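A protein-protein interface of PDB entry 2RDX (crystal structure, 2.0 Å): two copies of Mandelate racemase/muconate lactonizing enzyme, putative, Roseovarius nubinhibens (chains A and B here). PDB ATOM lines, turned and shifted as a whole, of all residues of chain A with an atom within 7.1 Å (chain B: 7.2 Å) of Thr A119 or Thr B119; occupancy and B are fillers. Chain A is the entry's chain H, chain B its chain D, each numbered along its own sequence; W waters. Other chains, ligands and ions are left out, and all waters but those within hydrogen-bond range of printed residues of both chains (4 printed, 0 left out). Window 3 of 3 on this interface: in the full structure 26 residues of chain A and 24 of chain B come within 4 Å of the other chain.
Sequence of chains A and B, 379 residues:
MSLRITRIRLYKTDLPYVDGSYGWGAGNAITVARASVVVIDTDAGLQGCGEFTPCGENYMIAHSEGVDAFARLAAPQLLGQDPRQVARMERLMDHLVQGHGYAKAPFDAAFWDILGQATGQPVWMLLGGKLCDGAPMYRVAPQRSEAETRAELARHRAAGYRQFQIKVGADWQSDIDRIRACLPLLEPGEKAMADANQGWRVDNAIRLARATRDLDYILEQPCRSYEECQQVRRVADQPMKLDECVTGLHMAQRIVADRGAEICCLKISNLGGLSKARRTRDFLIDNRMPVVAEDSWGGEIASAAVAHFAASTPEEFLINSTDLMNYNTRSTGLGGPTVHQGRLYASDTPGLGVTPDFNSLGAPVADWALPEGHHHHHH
The backbone carbonyl oxygen (O) of Arg A84 lies close to the side-chain sulfur (SD) of Met B125, at 3.5 Å.
The backbone carbonyl oxygen of Gln B121 sits at hydrogen-bond distance from the backbone NH of Gly B351 (2.9 Å). The backbone NH of Gln A121 is in hydrogen-bond range of the backbone carbonyl oxygen of Gly A116. The side-chain hydroxyl (OG1) of Thr B119 sits at hydrogen-bond distance from the backbone carbonyl oxygen (O) of Gly B116 (2.7 Å). The backbone NH (N) of Gln B121 is in hydrogen-bond range of the backbone carbonyl oxygen (O) of Gly B116 (2.9 Å). O of Leu A115 is in hydrogen-bond range of OG1 of Thr A119 (2.7 Å). O of Gln A121 is in hydrogen-bond range of N of Gly A351, at 3.0 Å.
O of Thr B119 touches CA of Thr A119, 3.7 Å away. CG2 of Thr A119 touches CG of Gln B121 (3.9 Å). NE2 of Gln A121 touches NH2 of Arg B84, at 3.6 Å. CG of Gln A121 touches CG2 of Thr B119, 3.9 Å away. Arg B84 touches Met A125.
Of the printed residues of chain B, Arg A84 touches Met B125. Of the printed residues of chain B, Thr A119 touches Thr B119 (3.7 Å) and Gln B121 (3.9 Å). Printed residues of chain B within 4 Å of Gln A121: Arg B84 (3.6 Å) and Thr B119 (3.9 Å). Printed residues of chain A within 4 Å of Arg B84: Gln A121 and Met A125. Printed residues of chain A within 4 Å of Thr B119: Thr A119 and Gln A121. Of the printed residues of chain A, Gln B121 touches Thr A119. Of the printed residues of chain A, Met B125 touches Arg A84 (3.5 Å). The nearest residue of chain B that does not touch Thr A119 is Ala B118 (4.2 Å). The nearest residue of chain A that does not touch Thr B119 is Ala A118 (4.1 Å).
Printed residues of chain A that touch a printed residue of chain B: Arg A84, Thr A119, Gln A121 and Met A125. Hydrophobic or aromatic side chains of chain A that line the printed part of chain B: Met A125. Among the printed residues, 6 pairs touch across the chains. Among the printed residues, no Asp or Glu carboxylate lies within 4 Å of a Lys or Arg side-chain nitrogen of the other chain.
Arg A84 touches Met B125, and with the chains exchanged Met A125 touches Arg B84. Thr B119 touches its own counterpart, Thr A119. Thr A119 touches Gln B121, and with the chains exchanged Gln A121 touches Thr B119. Gln A121 touches Arg B84, but with the chains exchanged Arg A84 does not touch Gln B121 (4.04 Å). Of the 6 pairs that touch across the chains among the printed residues, 5 have their exchanged pair printed and touching as well.
Water W3 bridges the backbone carbonyl oxygen of Arg A84 (2.6 Å) and the backbone carbonyl oxygen of Met B125 (2.6 Å). Water W4 lies within hydrogen-bond range of O of Ala A118 (2.6 Å), O of Thr B119 (2.7 Å) and NE2 of Gln B121 (2.9 Å). Water W2 bridges the backbone carbonyl oxygen (O) of Met A125 (2.7 Å) and the backbone carbonyl oxygen (O) of Arg B84 (2.7 Å). Water W1 bridges NH2 of Arg B84 (2.9 Å) and NE2 of Gln A121 (3.2 Å).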
ATOM      1  N   LEU A  46     -36.129   1.896 -36.716  1.00  0.00           N
ATOM      2  CA  LEU A  46     -35.998   2.566 -35.422  1.00  0.00           C
ATOM      3  C   LEU A  46     -37.082   3.628 -35.291  1.00  0.00           C
ATOM      4  O   LEU A  46     -37.194   4.516 -36.135  1.00  0.00           O
ATOM      5  CB  LEU A  46     -34.611   3.210 -35.257  1.00  0.00           C
ATOM      6  CG  LEU A  46     -33.363   2.322 -35.194  1.00  0.00           C
ATOM      7  CD1 LEU A  46     -32.121   3.179 -35.031  1.00  0.00           C
ATOM      8  CD2 LEU A  46     -33.449   1.298 -34.071  1.00  0.00           C
ATOM      9  N   ARG A  84     -31.064  11.330 -36.426  1.00  0.00           N
ATOM     10  CA  ARG A  84     -30.061  11.271 -35.367  1.00  0.00           C
ATOM     11  C   ARG A  84     -29.105  12.469 -35.344  1.00  0.00           C
ATOM     12  O   ARG A  84     -28.391  12.680 -34.364  1.00  0.00           O
ATOM     13  CB  ARG A  84     -29.347   9.916 -35.348  1.00  0.00           C
ATOM     14  CG  ARG A  84     -28.506   9.574 -36.542  1.00  0.00           C
ATOM     15  CD  ARG A  84     -28.814   8.160 -36.994  1.00  0.00           C
ATOM     16  NE  ARG A  84     -27.661   7.409 -37.486  1.00  0.00           N
ATOM     17  CZ  ARG A  84     -27.133   7.512 -38.704  1.00  0.00           C
ATOM     18  NH1 ARG A  84     -27.620   8.366 -39.589  1.00  0.00           N
ATOM     19  NH2 ARG A  84     -26.094   6.760 -39.035  1.00  0.00           N
ATOM     20  N   TRP A 112     -33.897  12.607 -30.409  1.00  0.00           N
ATOM     21  CA  TRP A 112     -32.987  12.182 -29.336  1.00  0.00           C
ATOM     22  C   TRP A 112     -33.182  10.717 -28.989  1.00  0.00           C
ATOM     23  O   TRP A 112     -32.209  10.008 -28.725  1.00  0.00           O
ATOM     24  CB  TRP A 112     -33.182  13.043 -28.087  1.00  0.00           C
ATOM     25  CG  TRP A 112     -32.414  14.342 -28.118  1.00  0.00           C
ATOM     26  CD1 TRP A 112     -32.901  15.576 -28.437  1.00  0.00           C
ATOM     27  CD2 TRP A 112     -31.023  14.526 -27.814  1.00  0.00           C
ATOM     28  NE1 TRP A 112     -31.905  16.516 -28.350  1.00  0.00           N
ATOM     29  CE2 TRP A 112     -30.741  15.902 -27.976  1.00  0.00           C
ATOM     30  CE3 TRP A 112     -29.987  13.658 -27.421  1.00  0.00           C
ATOM     31  CZ2 TRP A 112     -29.467  16.443 -27.754  1.00  0.00           C
ATOM     32  CZ3 TRP A 112     -28.721  14.188 -27.212  1.00  0.00           C
ATOM     33  CH2 TRP A 112     -28.470  15.571 -27.380  1.00  0.00           C
ATOM     34  N   ASP A 113     -34.446  10.285 -29.007  1.00  0.00           N
ATOM     35  CA  ASP A 113     -34.846   8.891 -28.804  1.00  0.00           C
ATOM     36  C   ASP A 113     -34.218   7.968 -29.836  1.00  0.00           C
ATOM     37  O   ASP A 113     -33.683   6.914 -29.481  1.00  0.00           O
ATOM     38  CB  ASP A 113     -36.372   8.779 -28.885  1.00  0.00           C
ATOM     39  CG  ASP A 113     -36.902   7.445 -28.395  1.00  0.00           C
ATOM     40  OD1 ASP A 113     -36.143   6.646 -27.805  1.00  0.00           O
ATOM     41  OD2 ASP A 113     -38.106   7.195 -28.607  1.00  0.00           O
ATOM     42  N   ILE A 114     -34.300   8.368 -31.103  1.00  0.00           N
ATOM     43  CA  ILE A 114     -33.764   7.596 -32.221  1.00  0.00           C
ATOM     44  C   ILE A 114     -32.240   7.519 -32.147  1.00  0.00           C
ATOM     45  O   ILE A 114     -31.659   6.442 -32.320  1.00  0.00           O
ATOM     46  CB  ILE A 114     -34.243   8.168 -33.583  1.00  0.00           C
ATOM     47  CG1 ILE A 114     -35.691   7.760 -33.826  1.00  0.00           C
ATOM     48  CG2 ILE A 114     -33.381   7.665 -34.743  1.00  0.00           C
ATOM     49  CD1 ILE A 114     -36.450   8.662 -34.784  1.00  0.00           C
ATOM     50  N   LEU A 115     -31.608   8.652 -31.844  1.00  0.00           N
ATOM     51  CA  LEU A 115     -30.150   8.719 -31.730  1.00  0.00           C
ATOM     52  C   LEU A 115     -29.637   7.754 -30.661  1.00  0.00           C
ATOM     53  O   LEU A 115     -28.644   7.057 -30.877  1.00  0.00           O
ATOM     54  CB  LEU A 115     -29.678  10.152 -31.438  1.00  0.00           C
ATOM     55  CG  LEU A 115     -28.198  10.342 -31.077  1.00  0.00           C
ATOM     56  CD1 LEU A 115     -27.265   9.990 -32.232  1.00  0.00           C
ATOM     57  CD2 LEU A 115     -27.936  11.746 -30.587  1.00  0.00           C
ATOM     58  N   GLY A 116     -30.337   7.721 -29.527  1.00  0.00           N
ATOM     59  CA  GLY A 116     -30.054   6.793 -28.430  1.00  0.00           C
ATOM     60  C   GLY A 116     -30.151   5.332 -28.812  1.00  0.00           C
ATOM     61  O   GLY A 116     -29.326   4.523 -28.396  1.00  0.00           O
ATOM     62  N   GLN A 117     -31.165   5.004 -29.607  1.00  0.00           N
ATOM     63  CA  GLN A 117     -31.343   3.662 -30.135  1.00  0.00           C
ATOM     64  C   GLN A 117     -30.232   3.284 -31.120  1.00  0.00           C
ATOM     65  O   GLN A 117     -29.670   2.198 -31.023  1.00  0.00           O
ATOM     66  CB  GLN A 117     -32.714   3.535 -30.789  1.00  0.00           C
ATOM     67  CG  GLN A 117     -33.880   3.538 -29.806  1.00  0.00           C
ATOM     68  CD  GLN A 117     -35.228   3.559 -30.499  1.00  0.00           C
ATOM     69  OE1 GLN A 117     -35.543   2.672 -31.299  1.00  0.00           O
ATOM     70  NE2 GLN A 117     -36.035   4.570 -30.196  1.00  0.00           N
ATOM     71  N   ALA A 118     -29.913   4.191 -32.047  1.00  0.00           N
ATOM     72  CA  ALA A 118     -28.834   3.990 -33.027  1.00  0.00           C
ATOM     73  C   ALA A 118     -27.425   3.887 -32.412  1.00  0.00           C
ATOM     74  O   ALA A 118     -26.549   3.224 -32.969  1.00  0.00           O
ATOM     75  CB  ALA A 118     -28.870   5.095 -34.079  1.00  0.00           C
ATOM     76  N   THR A 119     -27.216   4.556 -31.280  1.00  0.00           N
ATOM     77  CA  THR A 119     -25.948   4.496 -30.544  1.00  0.00           C
ATOM     78  C   THR A 119     -25.944   3.403 -29.477  1.00  0.00           C
ATOM     79  O   THR A 119     -24.891   3.082 -28.915  1.00  0.00           O
ATOM     80  CB  THR A 119     -25.630   5.841 -29.859  1.00  0.00           C
ATOM     81  OG1 THR A 119     -26.762   6.267 -29.096  1.00  0.00           O
ATOM     82  CG2 THR A 119     -25.277   6.916 -30.896  1.00  0.00           C
ATOM     83  N   GLY A 120     -27.117   2.829 -29.211  1.00  0.00           N
ATOM     84  CA  GLY A 120     -27.288   1.839 -28.146  1.00  0.00           C
ATOM     85  C   GLY A 120     -27.110   2.389 -26.736  1.00  0.00           C
ATOM     86  O   GLY A 120     -26.706   1.657 -25.823  1.00  0.00           O
ATOM     87  N   GLN A 121     -27.423   3.671 -26.554  1.00  0.00           N
ATOM     88  CA  GLN A 121     -27.185   4.376 -25.293  1.00  0.00           C
ATOM     89  C   GLN A 121     -28.426   5.136 -24.818  1.00  0.00           C
ATOM     90  O   GLN A 121     -29.177   5.656 -25.631  1.00  0.00           O
ATOM     91  CB  GLN A 121     -26.006   5.358 -25.433  1.00  0.00           C
ATOM     92  CG  GLN A 121     -24.610   4.714 -25.511  1.00  0.00           C
ATOM     93  CD  GLN A 121     -24.236   3.957 -24.249  1.00  0.00           C
ATOM     94  OE1 GLN A 121     -24.588   4.364 -23.146  1.00  0.00           O
ATOM     95  NE2 GLN A 121     -23.522   2.848 -24.407  1.00  0.00           N
ATOM     96  N   PRO A 122     -28.654   5.190 -23.494  1.00  0.00           N
ATOM     97  CA  PRO A 122     -29.706   6.036 -22.934  1.00  0.00           C
ATOM     98  C   PRO A 122     -29.452   7.507 -23.224  1.00  0.00           C
ATOM     99  O   PRO A 122     -28.297   7.910 -23.359  1.00  0.00           O
ATOM    100  CB  PRO A 122     -29.578   5.794 -21.432  1.00  0.00           C
ATOM    101  CG  PRO A 122     -28.184   5.294 -21.250  1.00  0.00           C
ATOM    102  CD  PRO A 122     -27.951   4.444 -22.438  1.00  0.00           C
ATOM    103  N   MET A 125     -26.732   9.518 -21.375  1.00  0.00           N
ATOM    104  CA  MET A 125     -25.358   9.339 -21.849  1.00  0.00           C
ATOM    105  C   MET A 125     -24.986  10.353 -22.943  1.00  0.00           C
ATOM    106  O   MET A 125     -23.906  10.953 -22.909  1.00  0.00           O
ATOM    107  CB  MET A 125     -25.130   7.898 -22.328  1.00  0.00           C
ATOM    108  CG  MET A 125     -23.693   7.591 -22.763  1.00  0.00           C
ATOM    109  SD  MET A 125     -22.505   7.693 -21.428  1.00  0.00           S
ATOM    110  CE  MET A 125     -22.739   6.102 -20.675  1.00  0.00           C
ATOM    111  N   LEU A 126     -25.899  10.568 -23.887  1.00  0.00           N
ATOM    112  CA  LEU A 126     -25.657  11.505 -24.996  1.00  0.00           C
ATOM    113  C   LEU A 126     -25.729  12.974 -24.559  1.00  0.00           C
ATOM    114  O   LEU A 126     -25.235  13.863 -25.254  1.00  0.00           O
ATOM    115  CB  LEU A 126     -26.624  11.238 -26.147  1.00  0.00           C
ATOM    116  CG  LEU A 126     -26.745   9.772 -26.566  1.00  0.00           C
ATOM    117  CD1 LEU A 126     -27.999   9.591 -27.370  1.00  0.00           C
ATOM    118  CD2 LEU A 126     -25.518   9.299 -27.339  1.00  0.00           C
ATOM    119  N   PRO A 350     -31.355   1.791 -24.230  1.00  0.00           N
ATOM    120  CA  PRO A 350     -31.123   2.756 -25.334  1.00  0.00           C
ATOM    121  C   PRO A 350     -32.315   3.656 -25.658  1.00  0.00           C
ATOM    122  O   PRO A 350     -33.457   3.200 -25.624  1.00  0.00           O
ATOM    123  CB  PRO A 350     -30.829   1.852 -26.538  1.00  0.00           C
ATOM    124  CG  PRO A 350     -30.340   0.573 -25.940  1.00  0.00           C
ATOM    125  CD  PRO A 350     -31.140   0.399 -24.686  1.00  0.00           C
ATOM    126  N   GLY A 351     -32.040   4.925 -25.973  1.00  0.00           N
ATOM    127  CA  GLY A 351     -33.085   5.900 -26.312  1.00  0.00           C
ATOM    128  C   GLY A 351     -33.753   6.499 -25.088  1.00  0.00           C
ATOM    129  O   GLY A 351     -33.172   6.512 -24.003  1.00  0.00           O
ATOM    130  N   LEU B  46     -11.241  -0.529 -25.711  1.00  0.00           N
ATOM    131  CA  LEU B  46     -11.396   0.705 -26.467  1.00  0.00           C
ATOM    132  C   LEU B  46     -10.305   1.671 -26.032  1.00  0.00           C
ATOM    133  O   LEU B  46     -10.104   1.902 -24.836  1.00  0.00           O
ATOM    134  CB  LEU B  46     -12.783   1.336 -26.254  1.00  0.00           C
ATOM    135  CG  LEU B  46     -14.069   0.574 -26.605  1.00  0.00           C
ATOM    136  CD1 LEU B  46     -15.266   1.461 -26.338  1.00  0.00           C
ATOM    137  CD2 LEU B  46     -14.083   0.097 -28.054  1.00  0.00           C
ATOM    138  N   ARG B  84     -16.794   7.318 -21.099  1.00  0.00           N
ATOM    139  CA  ARG B  84     -17.882   7.611 -22.036  1.00  0.00           C
ATOM    140  C   ARG B  84     -18.691   8.799 -21.545  1.00  0.00           C
ATOM    141  O   ARG B  84     -19.248   9.561 -22.341  1.00  0.00           O
ATOM    142  CB  ARG B  84     -18.799   6.399 -22.192  1.00  0.00           C
ATOM    143  CG  ARG B  84     -18.119   5.162 -22.771  1.00  0.00           C
ATOM    144  CD  ARG B  84     -19.017   3.937 -22.704  1.00  0.00           C
ATOM    145  NE  ARG B  84     -19.548   3.720 -21.360  1.00  0.00           N
ATOM    146  CZ  ARG B  84     -20.491   2.837 -21.045  1.00  0.00           C
ATOM    147  NH1 ARG B  84     -20.904   2.739 -19.789  1.00  0.00           N
ATOM    148  NH2 ARG B  84     -21.025   2.054 -21.975  1.00  0.00           N
ATOM    149  N   TRP B 112     -14.063  11.781 -25.619  1.00  0.00           N
ATOM    150  CA  TRP B 112     -14.986  11.914 -26.755  1.00  0.00           C
ATOM    151  C   TRP B 112     -14.743  10.824 -27.792  1.00  0.00           C
ATOM    152  O   TRP B 112     -15.691  10.291 -28.384  1.00  0.00           O
ATOM    153  CB  TRP B 112     -14.865  13.304 -27.413  1.00  0.00           C
ATOM    154  CG  TRP B 112     -15.661  14.394 -26.724  1.00  0.00           C
ATOM    155  CD1 TRP B 112     -15.191  15.306 -25.831  1.00  0.00           C
ATOM    156  CD2 TRP B 112     -17.059  14.675 -26.882  1.00  0.00           C
ATOM    157  NE1 TRP B 112     -16.203  16.127 -25.411  1.00  0.00           N
ATOM    158  CE2 TRP B 112     -17.359  15.770 -26.044  1.00  0.00           C
ATOM    159  CE3 TRP B 112     -18.082  14.113 -27.653  1.00  0.00           C
ATOM    160  CZ2 TRP B 112     -18.645  16.317 -25.949  1.00  0.00           C
ATOM    161  CZ3 TRP B 112     -19.365  14.650 -27.552  1.00  0.00           C
ATOM    162  CH2 TRP B 112     -19.631  15.741 -26.704  1.00  0.00           C
ATOM    163  N   ASP B 113     -13.466  10.506 -27.999  1.00  0.00           N
ATOM    164  CA  ASP B 113     -13.022   9.463 -28.932  1.00  0.00           C
ATOM    165  C   ASP B 113     -13.601   8.102 -28.522  1.00  0.00           C
ATOM    166  O   ASP B 113     -14.195   7.395 -29.343  1.00  0.00           O
ATOM    167  CB  ASP B 113     -11.486   9.440 -28.940  1.00  0.00           C
ATOM    168  CG  ASP B 113     -10.898   8.489 -29.963  1.00  0.00           C
ATOM    169  OD1 ASP B 113     -11.597   8.033 -30.893  1.00  0.00           O
ATOM    170  OD2 ASP B 113      -9.693   8.210 -29.837  1.00  0.00           O
ATOM    171  N   ILE B 114     -13.435   7.768 -27.242  1.00  0.00           N
ATOM    172  CA  ILE B 114     -13.951   6.545 -26.641  1.00  0.00           C
ATOM    173  C   ILE B 114     -15.480   6.455 -26.722  1.00  0.00           C
ATOM    174  O   ILE B 114     -16.024   5.387 -27.037  1.00  0.00           O
ATOM    175  CB  ILE B 114     -13.445   6.399 -25.173  1.00  0.00           C
ATOM    176  CG1 ILE B 114     -11.982   5.947 -25.177  1.00  0.00           C
ATOM    177  CG2 ILE B 114     -14.300   5.403 -24.392  1.00  0.00           C
ATOM    178  CD1 ILE B 114     -11.198   6.305 -23.925  1.00  0.00           C
ATOM    179  N   LEU B 115     -16.158   7.573 -26.453  1.00  0.00           N
ATOM    180  CA  LEU B 115     -17.616   7.658 -26.582  1.00  0.00           C
ATOM    181  C   LEU B 115     -18.047   7.386 -28.022  1.00  0.00           C
ATOM    182  O   LEU B 115     -18.972   6.611 -28.254  1.00  0.00           O
ATOM    183  CB  LEU B 115     -18.142   9.024 -26.112  1.00  0.00           C
ATOM    184  CG  LEU B 115     -19.659   9.266 -26.214  1.00  0.00           C
ATOM    185  CD1 LEU B 115     -20.495   8.232 -25.442  1.00  0.00           C
ATOM    186  CD2 LEU B 115     -20.022  10.674 -25.780  1.00  0.00           C
ATOM    187  N   GLY B 116     -17.359   8.009 -28.980  1.00  0.00           N
ATOM    188  CA  GLY B 116     -17.597   7.754 -30.399  1.00  0.00           C
ATOM    189  C   GLY B 116     -17.553   6.279 -30.737  1.00  0.00           C
ATOM    190  O   GLY B 116     -18.508   5.732 -31.298  1.00  0.00           O
ATOM    191  N   GLN B 117     -16.441   5.647 -30.359  1.00  0.00           N
ATOM    192  CA  GLN B 117     -16.174   4.229 -30.580  1.00  0.00           C
ATOM    193  C   GLN B 117     -17.198   3.325 -29.912  1.00  0.00           C
ATOM    194  O   GLN B 117     -17.617   2.321 -30.489  1.00  0.00           O
ATOM    195  CB  GLN B 117     -14.795   3.874 -30.035  1.00  0.00           C
ATOM    196  CG  GLN B 117     -13.641   4.404 -30.855  1.00  0.00           C
ATOM    197  CD  GLN B 117     -12.304   4.062 -30.242  1.00  0.00           C
ATOM    198  OE1 GLN B 117     -12.018   2.895 -29.958  1.00  0.00           O
ATOM    199  NE2 GLN B 117     -11.473   5.078 -30.031  1.00  0.00           N
ATOM    200  N   ALA B 118     -17.588   3.694 -28.690  1.00  0.00           N
ATOM    201  CA  ALA B 118     -18.580   2.963 -27.905  1.00  0.00           C
ATOM    202  C   ALA B 118     -19.977   3.025 -28.523  1.00  0.00           C
ATOM    203  O   ALA B 118     -20.798   2.133 -28.309  1.00  0.00           O
ATOM    204  CB  ALA B 118     -18.613   3.501 -26.480  1.00  0.00           C
ATOM    205  N   THR B 119     -20.232   4.081 -29.291  1.00  0.00           N
ATOM    206  CA  THR B 119     -21.538   4.326 -29.902  1.00  0.00           C
ATOM    207  C   THR B 119     -21.564   4.007 -31.401  1.00  0.00           C
ATOM    208  O   THR B 119     -22.629   4.040 -32.036  1.00  0.00           O
ATOM    209  CB  THR B 119     -21.922   5.796 -29.730  1.00  0.00           C
ATOM    210  OG1 THR B 119     -20.831   6.613 -30.164  1.00  0.00           O
ATOM    211  CG2 THR B 119     -22.236   6.109 -28.264  1.00  0.00           C
ATOM    212  N   GLY B 120     -20.390   3.709 -31.958  1.00  0.00           N
ATOM    213  CA  GLY B 120     -20.223   3.470 -33.395  1.00  0.00           C
ATOM    214  C   GLY B 120     -20.446   4.694 -34.269  1.00  0.00           C
ATOM    215  O   GLY B 120     -20.889   4.569 -35.410  1.00  0.00           O
ATOM    216  N   GLN B 121     -20.140   5.873 -33.731  1.00  0.00           N
ATOM    217  CA  GLN B 121     -20.406   7.143 -34.415  1.00  0.00           C
ATOM    218  C   GLN B 121     -19.195   8.081 -34.400  1.00  0.00           C
ATOM    219  O   GLN B 121     -18.448   8.104 -33.426  1.00  0.00           O
ATOM    220  CB  GLN B 121     -21.615   7.864 -33.792  1.00  0.00           C
ATOM    221  CG  GLN B 121     -22.981   7.215 -34.049  1.00  0.00           C
ATOM    222  CD  GLN B 121     -23.285   6.976 -35.525  1.00  0.00           C
ATOM    223  OE1 GLN B 121     -23.035   7.829 -36.377  1.00  0.00           O
ATOM    224  NE2 GLN B 121     -23.837   5.808 -35.827  1.00  0.00           N
ATOM    225  N   PRO B 122     -18.989   8.848 -35.493  1.00  0.00           N
ATOM    226  CA  PRO B 122     -17.954   9.879 -35.503  1.00  0.00           C
ATOM    227  C   PRO B 122     -18.292  10.969 -34.498  1.00  0.00           C
ATOM    228  O   PRO B 122     -19.472  11.207 -34.218  1.00  0.00           O
ATOM    229  CB  PRO B 122     -18.031  10.433 -36.921  1.00  0.00           C
ATOM    230  CG  PRO B 122     -19.405  10.104 -37.378  1.00  0.00           C
ATOM    231  CD  PRO B 122     -19.698   8.784 -36.783  1.00  0.00           C
ATOM    232  N   MET B 125     -21.169  13.529 -34.976  1.00  0.00           N
ATOM    233  CA  MET B 125     -22.548  13.070 -34.749  1.00  0.00           C
ATOM    234  C   MET B 125     -22.954  13.364 -33.314  1.00  0.00           C
ATOM    235  O   MET B 125     -24.031  13.898 -33.057  1.00  0.00           O
ATOM    236  CB  MET B 125     -22.701  11.570 -35.070  1.00  0.00           C
ATOM    237  CG  MET B 125     -24.141  11.007 -34.901  1.00  0.00           C
ATOM    238  SD  MET B 125     -25.396  11.716 -35.990  1.00  0.00           S
ATOM    239  CE  MET B 125     -25.092  10.730 -37.452  1.00  0.00           C
ATOM    240  N   LEU B 126     -22.049  13.051 -32.394  1.00  0.00           N
ATOM    241  CA  LEU B 126     -22.251  13.278 -30.969  1.00  0.00           C
ATOM    242  C   LEU B 126     -22.219  14.749 -30.568  1.00  0.00           C
ATOM    243  O   LEU B 126     -22.684  15.100 -29.483  1.00  0.00           O
ATOM    244  CB  LEU B 126     -21.212  12.505 -30.166  1.00  0.00           C
ATOM    245  CG  LEU B 126     -21.134  10.999 -30.410  1.00  0.00           C
ATOM    246  CD1 LEU B 126     -19.845  10.518 -29.810  1.00  0.00           C
ATOM    247  CD2 LEU B 126     -22.347  10.255 -29.827  1.00  0.00           C
ATOM    248  N   PRO B 350     -16.174   5.688 -36.600  1.00  0.00           N
ATOM    249  CA  PRO B 350     -16.378   5.912 -35.147  1.00  0.00           C
ATOM    250  C   PRO B 350     -15.235   6.588 -34.387  1.00  0.00           C
ATOM    251  O   PRO B 350     -14.062   6.310 -34.641  1.00  0.00           O
ATOM    252  CB  PRO B 350     -16.591   4.493 -34.600  1.00  0.00           C
ATOM    253  CG  PRO B 350     -17.154   3.748 -35.731  1.00  0.00           C
ATOM    254  CD  PRO B 350     -16.465   4.287 -36.958  1.00  0.00           C
ATOM    255  N   GLY B 351     -15.590   7.478 -33.463  1.00  0.00           N
ATOM    256  CA  GLY B 351     -14.596   8.179 -32.652  1.00  0.00           C
ATOM    257  C   GLY B 351     -14.002   9.404 -33.326  1.00  0.00           C
ATOM    258  O   GLY B 351     -14.657  10.056 -34.147  1.00  0.00           O
HETATM  259  O   HOH W   1     -23.114   0.173 -22.791  1.00  0.00           O
HETATM  260  O   HOH W   2     -21.288  11.345 -22.650  1.00  0.00           O
HETATM  261  O   HOH W   3     -26.654  14.028 -32.934  1.00  0.00           O
HETATM  262  O   HOH W   4     -24.207   3.493 -34.153  1.00  0.00           O
